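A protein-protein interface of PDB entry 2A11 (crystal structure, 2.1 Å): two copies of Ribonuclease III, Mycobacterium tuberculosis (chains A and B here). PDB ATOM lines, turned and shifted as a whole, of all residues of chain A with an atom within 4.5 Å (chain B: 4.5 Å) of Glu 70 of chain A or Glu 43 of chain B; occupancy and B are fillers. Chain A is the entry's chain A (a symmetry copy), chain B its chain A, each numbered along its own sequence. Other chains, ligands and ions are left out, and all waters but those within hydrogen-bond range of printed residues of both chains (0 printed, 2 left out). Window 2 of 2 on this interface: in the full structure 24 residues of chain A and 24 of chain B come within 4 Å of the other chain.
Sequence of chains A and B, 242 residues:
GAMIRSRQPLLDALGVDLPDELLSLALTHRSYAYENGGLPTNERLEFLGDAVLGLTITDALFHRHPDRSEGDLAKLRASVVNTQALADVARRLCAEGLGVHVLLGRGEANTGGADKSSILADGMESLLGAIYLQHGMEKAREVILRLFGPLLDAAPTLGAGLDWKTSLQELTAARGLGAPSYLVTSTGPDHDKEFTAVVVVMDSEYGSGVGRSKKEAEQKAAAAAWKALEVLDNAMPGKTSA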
ATOM      1  N   ARG A  68      28.917  21.854  14.033  1.00  0.00           N
ATOM      2  CA  ARG A  68      29.022  22.632  15.260  1.00  0.00           C
ATOM      3  C   ARG A  68      27.870  23.624  15.435  1.00  0.00           C
ATOM      4  O   ARG A  68      27.381  24.201  14.467  1.00  0.00           O
ATOM      5  CB  ARG A  68      30.379  23.332  15.308  1.00  0.00           C
ATOM      6  CG  ARG A  68      31.510  22.406  15.783  1.00  0.00           C
ATOM      7  CD  ARG A  68      32.833  22.746  15.125  1.00  0.00           C
ATOM      8  NE  ARG A  68      33.983  22.518  15.995  1.00  0.00           N
ATOM      9  CZ  ARG A  68      34.117  23.050  17.206  1.00  0.00           C
ATOM     10  NH1 ARG A  68      33.167  23.835  17.696  1.00  0.00           N
ATOM     11  NH2 ARG A  68      35.214  22.825  17.913  1.00  0.00           N
ATOM     12  N   SER A  69      27.442  23.796  16.683  1.00  0.00           N
ATOM     13  CA  SER A  69      26.326  24.667  17.038  1.00  0.00           C
ATOM     14  C   SER A  69      26.611  26.159  16.913  1.00  0.00           C
ATOM     15  O   SER A  69      27.763  26.589  16.910  1.00  0.00           O
ATOM     16  CB  SER A  69      25.892  24.380  18.479  1.00  0.00           C
ATOM     17  OG  SER A  69      26.830  24.931  19.402  1.00  0.00           O
ATOM     18  N   GLU A  70      25.547  26.951  16.846  1.00  0.00           N
ATOM     19  CA  GLU A  70      25.718  28.385  16.747  1.00  0.00           C
ATOM     20  C   GLU A  70      26.688  28.846  17.826  1.00  0.00           C
ATOM     21  O   GLU A  70      27.668  29.531  17.536  1.00  0.00           O
ATOM     22  CB  GLU A  70      24.379  29.102  16.909  1.00  0.00           C
ATOM     23  CG  GLU A  70      24.473  30.398  17.710  1.00  0.00           C
ATOM     24  CD  GLU A  70      23.247  31.280  17.562  1.00  0.00           C
ATOM     25  OE1 GLU A  70      22.110  30.761  17.657  1.00  0.00           O
ATOM     26  OE2 GLU A  70      23.422  32.501  17.353  1.00  0.00           O
ATOM     27  N   GLY A  71      26.408  28.451  19.068  1.00  0.00           N
ATOM     28  CA  GLY A  71      27.241  28.832  20.196  1.00  0.00           C
ATOM     29  C   GLY A  71      28.704  28.537  19.970  1.00  0.00           C
ATOM     30  O   GLY A  71      29.563  29.380  20.221  1.00  0.00           O
ATOM     31  N   ASP A  72      28.996  27.332  19.505  1.00  0.00           N
ATOM     32  CA  ASP A  72      30.375  26.962  19.241  1.00  0.00           C
ATOM     33  C   ASP A  72      30.926  27.844  18.128  1.00  0.00           C
ATOM     34  O   ASP A  72      32.046  28.350  18.223  1.00  0.00           O
ATOM     35  CB  ASP A  72      30.479  25.488  18.834  1.00  0.00           C
ATOM     36  CG  ASP A  72      30.450  24.539  20.031  1.00  0.00           C
ATOM     37  OD1 ASP A  72      30.264  25.017  21.174  1.00  0.00           O
ATOM     38  OD2 ASP A  72      30.626  23.316  19.830  1.00  0.00           O
ATOM     39  N   LEU A  73      30.136  28.022  17.072  1.00  0.00           N
ATOM     40  CA  LEU A  73      30.555  28.849  15.964  1.00  0.00           C
ATOM     41  C   LEU A  73      30.874  30.250  16.495  1.00  0.00           C
ATOM     42  O   LEU A  73      31.887  30.831  16.130  1.00  0.00           O
ATOM     43  CB  LEU A  73      29.465  28.893  14.898  1.00  0.00           C
ATOM     44  CG  LEU A  73      29.308  27.615  14.066  1.00  0.00           C
ATOM     45  CD1 LEU A  73      28.235  27.814  12.990  1.00  0.00           C
ATOM     46  CD2 LEU A  73      30.638  27.272  13.409  1.00  0.00           C
ATOM     47  N   ALA A  74      30.032  30.782  17.373  1.00  0.00           N
ATOM     48  CA  ALA A  74      30.289  32.103  17.928  1.00  0.00           C
ATOM     49  C   ALA A  74      31.613  32.110  18.696  1.00  0.00           C
ATOM     50  O   ALA A  74      32.339  33.108  18.703  1.00  0.00           O
ATOM     51  CB  ALA A  74      29.163  32.516  18.844  1.00  0.00           C
ATOM     52  N   ARG B  30      14.189  25.674  17.657  1.00  0.00           N
ATOM     53  CA  ARG B  30      14.731  24.648  18.535  1.00  0.00           C
ATOM     54  C   ARG B  30      13.687  23.830  19.313  1.00  0.00           C
ATOM     55  O   ARG B  30      13.878  22.633  19.531  1.00  0.00           O
ATOM     56  CB  ARG B  30      15.734  25.281  19.504  1.00  0.00           C
ATOM     57  CG  ARG B  30      15.117  26.268  20.481  1.00  0.00           C
ATOM     58  CD  ARG B  30      16.045  27.447  20.702  1.00  0.00           C
ATOM     59  NE  ARG B  30      17.150  27.101  21.584  1.00  0.00           N
ATOM     60  CZ  ARG B  30      17.047  26.279  22.624  1.00  0.00           C
ATOM     61  NH1 ARG B  30      17.698  25.121  22.621  1.00  0.00           N
ATOM     62  NH2 ARG B  30      16.283  26.609  23.662  1.00  0.00           N
ATOM     63  N   THR B  41      18.484  22.496  13.999  1.00  0.00           N
ATOM     64  CA  THR B  41      17.676  23.708  14.154  1.00  0.00           C
ATOM     65  C   THR B  41      18.115  24.819  13.215  1.00  0.00           C
ATOM     66  O   THR B  41      19.164  24.736  12.605  1.00  0.00           O
ATOM     67  CB  THR B  41      17.781  24.278  15.576  1.00  0.00           C
ATOM     68  OG1 THR B  41      19.087  24.839  15.761  1.00  0.00           O
ATOM     69  CG2 THR B  41      17.566  23.177  16.599  1.00  0.00           C
ATOM     70  N   ASN B  42      17.315  25.872  13.133  1.00  0.00           N
ATOM     71  CA  ASN B  42      17.649  27.011  12.286  1.00  0.00           C
ATOM     72  C   ASN B  42      18.680  27.950  12.927  1.00  0.00           C
ATOM     73  O   ASN B  42      18.957  29.012  12.386  1.00  0.00           O
ATOM     74  CB  ASN B  42      16.408  27.822  11.975  1.00  0.00           C
ATOM     75  CG  ASN B  42      15.828  28.505  13.212  1.00  0.00           C
ATOM     76  OD1 ASN B  42      16.395  28.435  14.308  1.00  0.00           O
ATOM     77  ND2 ASN B  42      14.692  29.174  13.034  1.00  0.00           N
ATOM     78  N   GLU B  43      19.261  27.553  14.057  1.00  0.00           N
ATOM     79  CA  GLU B  43      20.223  28.406  14.759  1.00  0.00           C
ATOM     80  C   GLU B  43      21.514  28.750  14.022  1.00  0.00           C
ATOM     81  O   GLU B  43      21.980  29.882  14.124  1.00  0.00           O
ATOM     82  CB  GLU B  43      20.537  27.809  16.140  1.00  0.00           C
ATOM     83  CG  GLU B  43      19.298  27.844  17.049  1.00  0.00           C
ATOM     84  CD  GLU B  43      19.470  27.052  18.320  1.00  0.00           C
ATOM     85  OE1 GLU B  43      19.559  25.805  18.236  1.00  0.00           O
ATOM     86  OE2 GLU B  43      19.519  27.683  19.398  1.00  0.00           O
ATOM     87  N   ARG B  44      22.085  27.798  13.283  1.00  0.00           N
ATOM     88  CA  ARG B  44      23.318  28.052  12.527  1.00  0.00           C
ATOM     89  C   ARG B  44      22.999  29.044  11.413  1.00  0.00           C
ATOM     90  O   ARG B  44      23.742  30.015  11.174  1.00  0.00           O
ATOM     91  CB  ARG B  44      23.870  26.744  11.950  1.00  0.00           C
ATOM     92  CG  ARG B  44      24.581  25.843  12.989  1.00  0.00           C
ATOM     93  CD  ARG B  44      24.776  24.428  12.433  1.00  0.00           C
ATOM     94  NE  ARG B  44      25.268  24.446  11.056  1.00  0.00           N
ATOM     95  CZ  ARG B  44      26.537  24.642  10.716  1.00  0.00           C
ATOM     96  NH1 ARG B  44      27.457  24.829  11.654  1.00  0.00           N
ATOM     97  NH2 ARG B  44      26.880  24.661   9.439  1.00  0.00           N
ATOM     98  N   LEU B  45      21.864  28.806  10.766  1.00  0.00           N
ATOM     99  CA  LEU B  45      21.380  29.662   9.695  1.00  0.00           C
ATOM    100  C   LEU B  45      21.148  31.092  10.228  1.00  0.00           C
ATOM    101  O   LEU B  45      21.462  32.085   9.564  1.00  0.00           O
ATOM    102  CB  LEU B  45      20.075  29.068   9.128  1.00  0.00           C
ATOM    103  CG  LEU B  45      20.002  28.449   7.722  1.00  0.00           C
ATOM    104  CD1 LEU B  45      21.381  28.271   7.105  1.00  0.00           C
ATOM    105  CD2 LEU B  45      19.228  27.142   7.799  1.00  0.00           C
ATOM    106  N   GLU B  46      20.593  31.192  11.432  1.00  0.00           N
ATOM    107  CA  GLU B  46      20.334  32.491  12.073  1.00  0.00           C
ATOM    108  C   GLU B  46      21.658  33.261  12.249  1.00  0.00           C
ATOM    109  O   GLU B  46      21.755  34.447  11.946  1.00  0.00           O
ATOM    110  CB  GLU B  46      19.698  32.257  13.456  1.00  0.00           C
ATOM    111  CG  GLU B  46      19.526  33.505  14.296  1.00  0.00           C
ATOM    112  CD  GLU B  46      19.501  33.197  15.786  1.00  0.00           C
ATOM    113  OE1 GLU B  46      18.924  32.162  16.172  1.00  0.00           O
ATOM    114  OE2 GLU B  46      20.051  33.990  16.571  1.00  0.00           O
ATOM    115  N   PHE B  47      22.654  32.555  12.750  1.00  0.00           N
ATOM    116  CA  PHE B  47      24.005  33.072  12.991  1.00  0.00           C
ATOM    117  C   PHE B  47      24.572  33.615  11.686  1.00  0.00           C
ATOM    118  O   PHE B  47      25.155  34.702  11.631  1.00  0.00           O
ATOM    119  CB  PHE B  47      24.877  31.916  13.475  1.00  0.00           C
ATOM    120  CG  PHE B  47      26.288  32.291  13.827  1.00  0.00           C
ATOM    121  CD1 PHE B  47      26.562  33.096  14.930  1.00  0.00           C
ATOM    122  CD2 PHE B  47      27.351  31.773  13.094  1.00  0.00           C
ATOM    123  CE1 PHE B  47      27.875  33.370  15.309  1.00  0.00           C
ATOM    124  CE2 PHE B  47      28.667  32.041  13.464  1.00  0.00           C
ATOM    125  CZ  PHE B  47      28.924  32.842  14.573  1.00  0.00           C
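Among the printed residues, pairs that only touch across the chains: Leu 73 of chain A with Arg 44 of chain B, Leu 73 of chain A with Phe 47 of chain B, Glu 70 of chain A with Glu 43 of chain B, Ala 74 of chain A with Phe 47 of chain B and Glu 70 of chain A with Glu 46 of chain B.
Printed residues of chain A that touch a printed residue of chain B: Arg 68, Glu 70, Leu 73 and Ala 74.
Hydrophobic or aromatic side chains of chain A that line the printed part of chain B: Leu 73 and Ala 74.
Along chain A the printed residues that touch a printed residue of chain B span positions 68 to 74.
Of the 8 printed residues of chain B, 4 touch a printed residue of chain A.
Printed residues of chain B that touch a printed residue of chain A: Glu 43, Arg 44, Glu 46 and Phe 47.
Hydrophobic or aromatic side chains of chain B within 4 Å of the printed part of chain A: Phe 47.
Among the printed residues, 6 pairs touch across the chains.
Among the printed residues, no Asp or Glu carboxylate lies within 4 Å of a Lys or Arg side-chain nitrogen of the other chain.
No position is printed for both chains.
Of the 6 pairs that touch across the chains among the printed residues, none has its exchanged pair printed and touching as well.
Of chain A, only Glu 70 comes within 4 Å of Glu 43 of chain B.
Of the printed residues of chain A, Phe 47 of chain B touches Leu 73 (3.6 Å) and Ala 74 (3.6 Å).
Printed residues of chain A within 4 Å of Arg 44 of chain B: Arg 68 and Leu 73.
Printed residues of chain B within 4 Å of Leu 73 of chain A: Arg 44 (3.4 Å) and Phe 47 (3.6 Å).
Printed residues of chain B within 4 Å of Arg 68 of chain A: Arg 44 (2.9 Å).
Of the printed residues of chain A, Glu 46 of chain B touches Glu 70 (3.8 Å).
Ser 69 of chain A touches none of the printed residues of chain B.
Leu 45 of chain B touches none of the printed residues of chain A.
The nearest printed residue of chain A that does not touch Phe 47 of chain B is Glu 70 of chain A (4.01 Å).
NE of Arg 30 of chain B lies within salt-bridge range of OE2 of Glu 43 of chain B, at 3.3 Å.
The side-chain hydroxyl (OG1) of Thr 41 of chain B sits at hydrogen-bond distance from the side-chain carboxylate (OE1) of Glu 43 of chain B (2.7 Å).
OD2 of Asp 72 of chain A is in salt-bridge range of NH1 of Arg 68 of chain A (3.4 Å).
O of Arg 68 of chain A lies within hydrogen-bond range of NH1 of Arg 44 of chain B, 2.9 Å away.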
